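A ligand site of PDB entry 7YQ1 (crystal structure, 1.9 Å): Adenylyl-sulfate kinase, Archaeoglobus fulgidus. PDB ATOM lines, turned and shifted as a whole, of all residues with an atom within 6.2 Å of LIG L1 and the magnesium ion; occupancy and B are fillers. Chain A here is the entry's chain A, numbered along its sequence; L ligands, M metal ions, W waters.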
ATOM      1  N   GLY A  12      -7.406   0.900   2.275  1.00  0.00           N
ATOM      2  CA  GLY A  12      -8.080   2.088   1.830  1.00  0.00           C
ATOM      3  C   GLY A  12      -9.558   2.093   2.133  1.00  0.00           C
ATOM      4  O   GLY A  12     -10.167   1.059   2.451  1.00  0.00           O
ATOM      5  N   PRO A  13     -10.188   3.267   2.037  1.00  0.00           N
ATOM      6  CA  PRO A  13     -11.634   3.369   2.275  1.00  0.00           C
ATOM      7  C   PRO A  13     -12.408   2.777   1.116  1.00  0.00           C
ATOM      8  O   PRO A  13     -11.863   2.401   0.076  1.00  0.00           O
ATOM      9  CB  PRO A  13     -11.867   4.877   2.405  1.00  0.00           C
ATOM     10  CG  PRO A  13     -10.773   5.490   1.607  1.00  0.00           C
ATOM     11  CD  PRO A  13      -9.574   4.585   1.755  1.00  0.00           C
ATOM     12  N   SER A  14     -13.724   2.700   1.310  1.00  0.00           N
ATOM     13  CA  SER A  14     -14.581   2.068   0.305  1.00  0.00           C
ATOM     14  C   SER A  14     -14.561   2.864  -0.986  1.00  0.00           C
ATOM     15  O   SER A  14     -14.673   4.089  -0.988  1.00  0.00           O
ATOM     16  CB  SER A  14     -16.007   1.959   0.836  1.00  0.00           C
ATOM     17  OG  SER A  14     -16.869   1.471  -0.170  1.00  0.00           O
ATOM     18  N   GLY A  15     -14.408   2.149  -2.106  1.00  0.00           N
ATOM     19  CA  GLY A  15     -14.361   2.791  -3.414  1.00  0.00           C
ATOM     20  C   GLY A  15     -13.007   3.325  -3.813  1.00  0.00           C
ATOM     21  O   GLY A  15     -12.897   3.957  -4.868  1.00  0.00           O
ATOM     22  N   ALA A  16     -11.978   3.092  -2.995  1.00  0.00           N
ATOM     23  CA  ALA A  16     -10.637   3.588  -3.323  1.00  0.00           C
ATOM     24  C   ALA A  16     -10.058   2.891  -4.548  1.00  0.00           C
ATOM     25  O   ALA A  16      -9.271   3.488  -5.282  1.00  0.00           O
ATOM     26  CB  ALA A  16      -9.711   3.408  -2.122  1.00  0.00           C
ATOM     27  N   GLY A  17     -10.426   1.633  -4.770  1.00  0.00           N
ATOM     28  CA  GLY A  17      -9.947   0.893  -5.928  1.00  0.00           C
ATOM     29  C   GLY A  17      -9.122  -0.318  -5.553  1.00  0.00           C
ATOM     30  O   GLY A  17      -8.329  -0.810  -6.371  1.00  0.00           O
ATOM     31  N   LYS A  18      -9.301  -0.812  -4.322  1.00  0.00           N
ATOM     32  CA  LYS A  18      -8.439  -1.865  -3.785  1.00  0.00           C
ATOM     33  C   LYS A  18      -8.592  -3.170  -4.575  1.00  0.00           C
ATOM     34  O   LYS A  18      -7.602  -3.776  -5.001  1.00  0.00           O
ATOM     35  CB  LYS A  18      -8.759  -2.111  -2.308  1.00  0.00           C
ATOM     36  CG  LYS A  18      -8.637  -0.904  -1.404  1.00  0.00           C
ATOM     37  CD  LYS A  18      -9.036  -1.235   0.038  1.00  0.00           C
ATOM     38  CE  LYS A  18     -10.454  -1.791   0.150  1.00  0.00           C
ATOM     39  NZ  LYS A  18     -11.500  -0.726   0.087  1.00  0.00           N
ATOM     40  N   THR A  19      -9.845  -3.611  -4.759  1.00  0.00           N
ATOM     41  CA  THR A  19     -10.080  -4.902  -5.404  1.00  0.00           C
ATOM     42  C   THR A  19      -9.684  -4.866  -6.873  1.00  0.00           C
ATOM     43  O   THR A  19      -9.125  -5.837  -7.399  1.00  0.00           O
ATOM     44  CB  THR A  19     -11.554  -5.292  -5.251  1.00  0.00           C
ATOM     45  OG1 THR A  19     -11.877  -5.348  -3.850  1.00  0.00           O
ATOM     46  CG2 THR A  19     -11.834  -6.650  -5.899  1.00  0.00           C
ATOM     47  N   THR A  20      -9.965  -3.744  -7.552  1.00  0.00           N
ATOM     48  CA  THR A  20      -9.540  -3.579  -8.938  1.00  0.00           C
ATOM     49  C   THR A  20      -8.033  -3.720  -9.079  1.00  0.00           C
ATOM     50  O   THR A  20      -7.542  -4.393  -9.989  1.00  0.00           O
ATOM     51  CB  THR A  20     -10.000  -2.224  -9.462  1.00  0.00           C
ATOM     52  OG1 THR A  20     -11.423  -2.110  -9.335  1.00  0.00           O
ATOM     53  CG2 THR A  20      -9.613  -2.052 -10.932  1.00  0.00           C
ATOM     54  N   LEU A  21      -7.276  -3.074  -8.189  1.00  0.00           N
ATOM     55  CA  LEU A  21      -5.826  -3.179  -8.269  1.00  0.00           C
ATOM     56  C   LEU A  21      -5.352  -4.583  -7.869  1.00  0.00           C
ATOM     57  O   LEU A  21      -4.433  -5.123  -8.489  1.00  0.00           O
ATOM     58  CB  LEU A  21      -5.162  -2.107  -7.408  1.00  0.00           C
ATOM     59  CG  LEU A  21      -3.642  -2.201  -7.357  1.00  0.00           C
ATOM     60  CD1 LEU A  21      -3.049  -1.959  -8.744  1.00  0.00           C
ATOM     61  CD2 LEU A  21      -3.084  -1.203  -6.350  1.00  0.00           C
ATOM     62  N   ASP A  40      -9.569 -11.017  -0.529  1.00  0.00           N
ATOM     63  CA  ASP A  40     -10.363  -9.812  -0.592  1.00  0.00           C
ATOM     64  C   ASP A  40     -11.313  -9.770   0.600  1.00  0.00           C
ATOM     65  O   ASP A  40     -11.938 -10.776   0.950  1.00  0.00           O
ATOM     66  CB  ASP A  40     -11.142  -9.730  -1.910  1.00  0.00           C
ATOM     67  CG  ASP A  40     -11.900  -8.410  -2.060  1.00  0.00           C
ATOM     68  OD1 ASP A  40     -11.242  -7.387  -2.327  1.00  0.00           O
ATOM     69  OD2 ASP A  40     -13.145  -8.408  -1.938  1.00  0.00           O
ATOM     70  N   ASP A  42     -14.266  -8.520   1.169  1.00  0.00           N
ATOM     71  CA  ASP A  42     -15.644  -8.915   0.921  1.00  0.00           C
ATOM     72  C   ASP A  42     -15.741 -10.404   0.607  1.00  0.00           C
ATOM     73  O   ASP A  42     -16.682 -11.082   1.059  1.00  0.00           O
ATOM     74  CB  ASP A  42     -16.226  -8.091  -0.222  1.00  0.00           C
ATOM     75  CG  ASP A  42     -17.723  -7.964  -0.128  1.00  0.00           C
ATOM     76  OD1 ASP A  42     -18.312  -8.685   0.684  1.00  0.00           O
ATOM     77  OD2 ASP A  42     -18.296  -7.094  -0.828  1.00  0.00           O
ATOM     78  N   SER A  83      -6.693  -7.372  -0.088  1.00  0.00           N
ATOM     79  CA  SER A  83      -7.460  -6.176  -0.433  1.00  0.00           C
ATOM     80  C   SER A  83      -8.576  -6.024   0.593  1.00  0.00           C
ATOM     81  O   SER A  83      -9.700  -6.491   0.414  1.00  0.00           O
ATOM     82  CB  SER A  83      -7.993  -6.237  -1.873  1.00  0.00           C
ATOM     83  OG  SER A  83      -8.787  -7.379  -2.098  1.00  0.00           O
ATOM     84  N   VAL A  85     -10.212  -3.194   3.771  1.00  0.00           N
ATOM     85  CA  VAL A  85     -10.274  -1.800   4.211  1.00  0.00           C
ATOM     86  C   VAL A  85      -9.166  -1.511   5.227  1.00  0.00           C
ATOM     87  O   VAL A  85      -8.366  -0.575   5.049  1.00  0.00           O
ATOM     88  CB  VAL A  85     -11.666  -1.474   4.781  1.00  0.00           C
ATOM     89  CG1 VAL A  85     -11.694  -0.075   5.361  1.00  0.00           C
ATOM     90  CG2 VAL A  85     -12.720  -1.621   3.686  1.00  0.00           C
ATOM     91  N   ARG A 117     -17.750   6.590  -7.878  1.00  0.00           N
ATOM     92  CA  ARG A 117     -17.197   5.303  -8.288  1.00  0.00           C
ATOM     93  C   ARG A 117     -17.731   4.195  -7.397  1.00  0.00           C
ATOM     94  O   ARG A 117     -16.967   3.426  -6.818  1.00  0.00           O
ATOM     95  CB  ARG A 117     -15.680   5.330  -8.222  1.00  0.00           C
ATOM     96  CG  ARG A 117     -15.019   6.380  -9.092  1.00  0.00           C
ATOM     97  CD  ARG A 117     -13.574   5.994  -9.293  1.00  0.00           C
ATOM     98  NE  ARG A 117     -12.832   6.898 -10.151  1.00  0.00           N
ATOM     99  CZ  ARG A 117     -11.506   7.001 -10.145  1.00  0.00           C
ATOM    100  NH1 ARG A 117     -10.776   6.288  -9.302  1.00  0.00           N
ATOM    101  NH2 ARG A 117     -10.916   7.831 -10.999  1.00  0.00           N
ATOM    102  N   ASP A 118     -19.064   4.104  -7.283  1.00  0.00           N
ATOM    103  CA  ASP A 118     -19.711   3.276  -6.266  1.00  0.00           C
ATOM    104  C   ASP A 118     -20.703   2.349  -6.939  1.00  0.00           C
ATOM    105  O   ASP A 118     -21.923   2.493  -6.764  1.00  0.00           O
ATOM    106  CB  ASP A 118     -20.373   4.177  -5.221  1.00  0.00           C
ATOM    107  CG  ASP A 118     -20.965   3.422  -4.057  1.00  0.00           C
ATOM    108  OD1 ASP A 118     -20.469   2.316  -3.727  1.00  0.00           O
ATOM    109  OD2 ASP A 118     -21.937   3.941  -3.459  1.00  0.00           O
ATOM    110  N   PRO A 119     -20.227   1.387  -7.742  1.00  0.00           N
ATOM    111  CA  PRO A 119     -21.156   0.509  -8.465  1.00  0.00           C
ATOM    112  C   PRO A 119     -21.980  -0.381  -7.549  1.00  0.00           C
ATOM    113  O   PRO A 119     -23.064  -0.808  -7.954  1.00  0.00           O
ATOM    114  CB  PRO A 119     -20.241  -0.333  -9.363  1.00  0.00           C
ATOM    115  CG  PRO A 119     -18.891  -0.225  -8.739  1.00  0.00           C
ATOM    116  CD  PRO A 119     -18.826   1.132  -8.122  1.00  0.00           C
ATOM    117  N   LYS A 120     -21.493  -0.659  -6.334  1.00  0.00           N
ATOM    118  CA  LYS A 120     -22.279  -1.391  -5.357  1.00  0.00           C
ATOM    119  C   LYS A 120     -23.271  -0.501  -4.616  1.00  0.00           C
ATOM    120  O   LYS A 120     -24.166  -1.027  -3.937  1.00  0.00           O
ATOM    121  CB  LYS A 120     -21.364  -2.079  -4.331  1.00  0.00           C
ATOM    122  CG  LYS A 120     -20.442  -3.136  -4.915  1.00  0.00           C
ATOM    123  CD  LYS A 120     -19.644  -3.806  -3.807  1.00  0.00           C
ATOM    124  CE  LYS A 120     -18.317  -3.080  -3.569  1.00  0.00           C
ATOM    125  NZ  LYS A 120     -17.330  -3.929  -2.854  1.00  0.00           N
ATOM    126  N   LEU A 122     -22.767   1.699  -2.043  1.00  0.00           N
ATOM    127  CA  LEU A 122     -22.621   1.759  -0.594  1.00  0.00           C
ATOM    128  C   LEU A 122     -22.758   3.186  -0.082  1.00  0.00           C
ATOM    129  O   LEU A 122     -23.353   3.410   0.980  1.00  0.00           O
ATOM    130  CB  LEU A 122     -21.271   1.166  -0.176  1.00  0.00           C
ATOM    131  CG  LEU A 122     -21.088  -0.329  -0.443  1.00  0.00           C
ATOM    132  CD1 LEU A 122     -19.644  -0.753  -0.221  1.00  0.00           C
ATOM    133  CD2 LEU A 122     -22.025  -1.134   0.439  1.00  0.00           C
ATOM    134  N   ASP A 152      -2.603   7.428  -6.667  1.00  0.00           N
ATOM    135  CA  ASP A 152      -3.766   8.305  -6.723  1.00  0.00           C
ATOM    136  C   ASP A 152      -4.679   7.775  -7.820  1.00  0.00           C
ATOM    137  O   ASP A 152      -4.456   8.039  -9.004  1.00  0.00           O
ATOM    138  CB  ASP A 152      -3.345   9.752  -6.961  1.00  0.00           C
ATOM    139  CG  ASP A 152      -2.611  10.340  -5.764  1.00  0.00           C
ATOM    140  OD1 ASP A 152      -3.291  10.679  -4.771  1.00  0.00           O
ATOM    141  OD2 ASP A 152      -1.376  10.463  -5.815  1.00  0.00           O
ATOM    142  N   THR A 153      -5.711   7.030  -7.428  1.00  0.00           N
ATOM    143  CA  THR A 153      -6.575   6.378  -8.397  1.00  0.00           C
ATOM    144  C   THR A 153      -7.498   7.351  -9.117  1.00  0.00           C
ATOM    145  O   THR A 153      -8.195   6.942 -10.047  1.00  0.00           O
ATOM    146  CB  THR A 153      -7.390   5.279  -7.726  1.00  0.00           C
ATOM    147  OG1 THR A 153      -8.325   5.844  -6.802  1.00  0.00           O
ATOM    148  CG2 THR A 153      -6.466   4.315  -6.991  1.00  0.00           C
ATOM    149  N   ASP A 154      -7.504   8.623  -8.728  1.00  0.00           N
ATOM    150  CA  ASP A 154      -8.178   9.650  -9.522  1.00  0.00           C
ATOM    151  C   ASP A 154      -7.251  10.274 -10.553  1.00  0.00           C
ATOM    152  O   ASP A 154      -7.722  11.035 -11.405  1.00  0.00           O
ATOM    153  CB  ASP A 154      -8.759  10.735  -8.597  1.00  0.00           C
ATOM    154  CG  ASP A 154      -7.687  11.471  -7.803  1.00  0.00           C
ATOM    155  OD1 ASP A 154      -6.814  10.806  -7.214  1.00  0.00           O
ATOM    156  OD2 ASP A 154      -7.747  12.715  -7.735  1.00  0.00           O
ATOM    157  N   MET A 156      -4.305   8.191 -11.837  1.00  0.00           N
ATOM    158  CA  MET A 156      -3.511   7.137 -12.447  1.00  0.00           C
ATOM    159  C   MET A 156      -4.430   6.044 -12.972  1.00  0.00           C
ATOM    160  O   MET A 156      -5.432   5.710 -12.346  1.00  0.00           O
ATOM    161  CB  MET A 156      -2.519   6.524 -11.450  1.00  0.00           C
ATOM    162  CG  MET A 156      -1.636   7.532 -10.755  1.00  0.00           C
ATOM    163  SD  MET A 156      -0.459   6.747  -9.636  1.00  0.00           S
ATOM    164  CE  MET A 156       0.306   5.536 -10.735  1.00  0.00           C
ATOM    165  N   THR A 157      -4.059   5.484 -14.126  1.00  0.00           N
ATOM    166  CA  THR A 157      -4.737   4.315 -14.648  1.00  0.00           C
ATOM    167  C   THR A 157      -4.364   3.084 -13.828  1.00  0.00           C
ATOM    168  O   THR A 157      -3.351   3.046 -13.137  1.00  0.00           O
ATOM    169  CB  THR A 157      -4.365   4.076 -16.113  1.00  0.00           C
ATOM    170  OG1 THR A 157      -2.975   3.702 -16.187  1.00  0.00           O
ATOM    171  CG2 THR A 157      -4.572   5.343 -16.932  1.00  0.00           C
ATOM    172  N   VAL A 158      -5.224   2.058 -13.911  1.00  0.00           N
ATOM    173  CA  VAL A 158      -4.924   0.784 -13.243  1.00  0.00           C
ATOM    174  C   VAL A 158      -3.598   0.235 -13.739  1.00  0.00           C
ATOM    175  O   VAL A 158      -2.782  -0.253 -12.945  1.00  0.00           O
ATOM    176  CB  VAL A 158      -6.073  -0.220 -13.462  1.00  0.00           C
ATOM    177  CG1 VAL A 158      -5.738  -1.542 -12.807  1.00  0.00           C
ATOM    178  CG2 VAL A 158      -7.375   0.351 -12.913  1.00  0.00           C
ATOM    179  N   GLU A 161      -0.891   1.943 -11.954  1.00  0.00           N
ATOM    180  CA  GLU A 161      -0.824   1.458 -10.574  1.00  0.00           C
ATOM    181  C   GLU A 161      -0.052   0.142 -10.493  1.00  0.00           C
ATOM    182  O   GLU A 161       0.807  -0.036  -9.631  1.00  0.00           O
ATOM    183  CB  GLU A 161      -2.224   1.293  -9.979  1.00  0.00           C
ATOM    184  CG  GLU A 161      -3.059   2.569  -9.930  1.00  0.00           C
ATOM    185  CD  GLU A 161      -4.495   2.291  -9.520  1.00  0.00           C
ATOM    186  OE1 GLU A 161      -4.729   1.324  -8.773  1.00  0.00           O
ATOM    187  OE2 GLU A 161      -5.393   3.042  -9.953  1.00  0.00           O
HETATM  188  P1  LIG L   1     -14.710  -1.762  -1.277  1.00  0.00           P
HETATM  189  O1  LIG L   1     -14.447  -3.216  -1.534  1.00  0.00           O
HETATM  190  O2  LIG L   1     -16.186  -1.537  -1.093  1.00  0.00           O
HETATM  191  O3  LIG L   1     -13.947  -1.309  -0.054  1.00  0.00           O
HETATM  192  P2  LIG L   1     -12.648  -1.023  -3.338  1.00  0.00           P
HETATM  193  O4  LIG L   1     -11.645  -0.223  -2.564  1.00  0.00           O
HETATM  194  O5  LIG L   1     -12.249  -2.498  -3.382  1.00  0.00           O
HETATM  195  N1  LIG L   1     -14.205  -0.821  -2.685  1.00  0.00           N
HETATM  196  P3  LIG L   1     -12.995  -1.162  -6.242  1.00  0.00           P
HETATM  197  O6  LIG L   1     -11.772  -1.962  -6.611  1.00  0.00           O
HETATM  198  O7  LIG L   1     -14.262  -2.017  -6.149  1.00  0.00           O
HETATM  199  O8  LIG L   1     -12.712  -0.363  -4.827  1.00  0.00           O
HETATM  200  O9  LIG L   1     -13.206   0.066  -7.331  1.00  0.00           O
HETATM  201  C1  LIG L   1     -14.412   0.818  -7.236  1.00  0.00           C
HETATM  202  C2  LIG L   1     -14.751   1.349  -8.608  1.00  0.00           C
HETATM  203  O10 LIG L   1     -13.574   2.359  -9.051  1.00  0.00           O
HETATM  204  C3  LIG L   1     -14.791   0.390  -9.514  1.00  0.00           C
HETATM  205  O11 LIG L   1     -15.852   0.705 -10.484  1.00  0.00           O
HETATM  206  C4  LIG L   1     -13.438   0.446 -10.260  1.00  0.00           C
HETATM  207  O12 LIG L   1     -13.593  -0.018 -11.531  1.00  0.00           O
HETATM  208  C5  LIG L   1     -13.197   1.972 -10.242  1.00  0.00           C
HETATM  209  N2  LIG L   1     -11.828   2.388 -10.490  1.00  0.00           N
HETATM  210  C6  LIG L   1     -11.041   1.552  -9.761  1.00  0.00           C
HETATM  211  N3  LIG L   1      -9.790   1.956  -9.996  1.00  0.00           N
HETATM  212  C7  LIG L   1      -9.828   3.014 -10.845  1.00  0.00           C
HETATM  213  C8  LIG L   1      -8.842   3.804 -11.403  1.00  0.00           C
HETATM  214  N4  LIG L   1      -7.379   3.890 -11.370  1.00  0.00           N
HETATM  215  N5  LIG L   1      -9.165   4.772 -12.202  1.00  0.00           N
HETATM  216  C9  LIG L   1     -10.475   5.027 -12.503  1.00  0.00           C
HETATM  217  N6  LIG L   1     -11.451   4.254 -11.959  1.00  0.00           N
HETATM  218  C10 LIG L   1     -11.108   3.267 -11.142  1.00  0.00           C
HETATM  219  S1  LG2 L   2     -12.736  -4.257   7.243  1.00  0.00           S
HETATM  220  O1  LG2 L   2     -13.432  -5.422   8.013  1.00  0.00           O
HETATM  221  O2  LG2 L   2     -12.704  -3.008   8.047  1.00  0.00           O
HETATM  222  O3  LG2 L   2     -11.252  -4.496   6.974  1.00  0.00           O
HETATM  223  P1  LG2 L   2     -13.621  -5.143   4.638  1.00  0.00           P
HETATM  224  O4  LG2 L   2     -13.697  -6.576   5.247  1.00  0.00           O
HETATM  225  O5  LG2 L   2     -12.484  -5.042   3.701  1.00  0.00           O
HETATM  226  O6  LG2 L   2     -13.512  -3.966   5.814  1.00  0.00           O
HETATM  227  O7  LG2 L   2     -15.044  -4.711   3.896  1.00  0.00           O
HETATM  228  C1  LG2 L   2     -15.802  -5.533   3.051  1.00  0.00           C
HETATM  229  C2  LG2 L   2     -16.805  -4.632   2.288  1.00  0.00           C
HETATM  230  O8  LG2 L   2     -17.777  -3.909   3.297  1.00  0.00           O
HETATM  231  C3  LG2 L   2     -16.229  -3.711   1.670  1.00  0.00           C
HETATM  232  O9  LG2 L   2     -16.958  -3.411   0.413  1.00  0.00           O
HETATM  233  C4  LG2 L   2     -16.392  -2.365   2.634  1.00  0.00           C
HETATM  234  O10 LG2 L   2     -16.083  -1.147   1.927  1.00  0.00           O
HETATM  235  C5  LG2 L   2     -17.603  -2.415   2.978  1.00  0.00           C
HETATM  236  N1  LG2 L   2     -17.708  -1.515   4.210  1.00  0.00           N
HETATM  237  C6  LG2 L   2     -16.898  -0.670   4.854  1.00  0.00           C
HETATM  238  N2  LG2 L   2     -17.573  -0.158   5.910  1.00  0.00           N
HETATM  239  C7  LG2 L   2     -18.795  -0.692   5.899  1.00  0.00           C
HETATM  240  C8  LG2 L   2     -19.865  -0.505   6.745  1.00  0.00           C
HETATM  241  N3  LG2 L   2     -20.109   0.305   7.955  1.00  0.00           N
HETATM  242  N4  LG2 L   2     -21.008  -1.160   6.544  1.00  0.00           N
HETATM  243  C9  LG2 L   2     -21.119  -1.998   5.500  1.00  0.00           C
HETATM  244  N5  LG2 L   2     -20.040  -2.189   4.634  1.00  0.00           N
HETATM  245  C10 LG2 L   2     -18.899  -1.533   4.849  1.00  0.00           C
HETATM  246 MG    MG M   1     -13.279  -4.157  -2.805  1.00  0.00          MG
HETATM  247  O   HOH W   1     -14.274  -6.007  -2.298  1.00  0.00           O
HETATM  248  O   HOH W   2     -14.624  -4.047  -4.420  1.00  0.00           O
HETATM  249  O   HOH W   3     -11.443   3.946  -7.492  1.00  0.00           O
HETATM  250  O   HOH W   4      -7.307   0.676  -8.686  1.00  0.00           O
HETATM  251  O   HOH W   5     -11.921  -4.569  -1.243  1.00  0.00           O
HETATM  252  O   HOH W   6     -16.665   3.423 -10.745  1.00  0.00           O
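The magnesium ion is bound by an oxygen (O1) of LIG L1.
The magnesium ion is bound by O5 of LIG L1, at 2.0 Å.
Water W2 binds the magnesium ion, 2.1 Å away.
The magnesium ion is bound by water W5 (2.1 Å).
OG1 of Thr 19 is bound to the magnesium ion (2.1 Å).
Water W1 binds the magnesium ion (2.2 Å).
The magnesium ion has six donor atoms within binding distance.
Water W5 lies within hydrogen-bond range of the side-chain carboxylate of Asp 40 and the backbone carbonyl oxygen of Ser 83.
Water W2 bridges an oxygen (O7) of LIG L1 (2.7 Å) and the side-chain amino group of Lys 120 (3.1 Å).
OG1 of Thr 153 lies within hydrogen-bond range of O of Ala 16 (3.0 Å).
The side-chain carboxylate of Asp 40 is in hydrogen-bond range of the side-chain hydroxyl of Ser 83, at 2.5 Å.
The side-chain carboxylate of Asp 40 sits close to the backbone NH of Asp 42.
O of Gly 12 is in hydrogen-bond range of NZ of Lys 18 (3.2 Å).
OD2 of Asp 42 is in salt-bridge range of NZ of Lys 120.
The backbone NH of Leu 122 lies within hydrogen-bond range of the side-chain carboxylate of Asp 118, at 2.8 Å.
The side-chain hydroxyl of Thr 19 lies close to the side-chain carboxylate of Asp 40, at 2.6 Å.
The guanidinium group (NH1) of Arg 117 lies within hydrogen-bond range of the backbone carbonyl oxygen (O) of Thr 153, 2.8 Å away.
N of Ala 16 sits at hydrogen-bond distance from O4 of LIG L1, at 3.4 Å.
The side-chain amino group of Lys 120 is in hydrogen-bond range of an oxygen (O9) of LG2 L2, 3.3 Å away.
N of Val 85 lies within hydrogen-bond range of O5 of LG2 L2 (2.9 Å).
OE2 of Glu 161 sits at hydrogen-bond distance from N4 of LIG L1 (2.6 Å).
O of Met 156 is in hydrogen-bond range of N4 of LIG L1 (2.8 Å).
The backbone NH (N) of Lys 18 lies within hydrogen-bond range of an oxygen (O4) of LIG L1 (3.0 Å).
The backbone carbonyl oxygen of Thr 153 lies within hydrogen-bond range of a nitrogen (N4) of LIG L1 (3.4 Å).
An oxygen (O6) of LIG L1 is in hydrogen-bond range of the side-chain hydroxyl (OG1) of Thr 20.
An oxygen (O10) of LG2 L2 lies close to the side-chain hydroxyl (OG) of Ser 14 (3.4 Å).
The side-chain amino group (NZ) of Lys 18 is in salt-bridge range of an oxygen (O3) of LIG L1.
OG of Ser 14 lies within hydrogen-bond range of O2 of LIG L1 (3.2 Å).
The backbone NH (N) of Thr 20 is in hydrogen-bond range of an oxygen (O6) of LIG L1, at 2.7 Å.
NH1 of Arg 117 sits close to N6 of LIG L1 (3.4 Å).
The backbone NH (N) of Gly 17 sits at hydrogen-bond distance from an oxygen (O8) of LIG L1 (3.0 Å).
O2 of LIG L1 is in salt-bridge range of NZ of Lys 120, 3.2 Å away.
O6 of LIG L1 sits at hydrogen-bond distance from N of Thr 19 (3.1 Å).
The backbone NH (N) of Gly 15 sits close to a nitrogen (N1) of LIG L1, 3.0 Å away.
Residues that only touch LIG L1: Pro 13, Val 85, Pro 119, Leu 122, Thr 157 and Val 158.
Hydrophobic or aromatic side chains that line LIG L1: Val 85, Pro 119, Leu 122 and Val 158.
Within 4 Å of LIG L1: Pro 13, Ser 14, Gly 15, Ala 16, Gly 17, Lys 18, Thr 19, Thr 20, Val 85, Arg 117, Pro 119, Lys 120, Leu 122, Thr 153, Met 156, Thr 157, Val 158 and Glu 161.
Along chain A the residues within 4 Å of LIG L1 span positions 13 to 161.
Asp 40 touches the magnesium ion.
O2 of LIG L1 is in hydrogen-bond range of O9 of LG2 L2 (2.5 Å).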
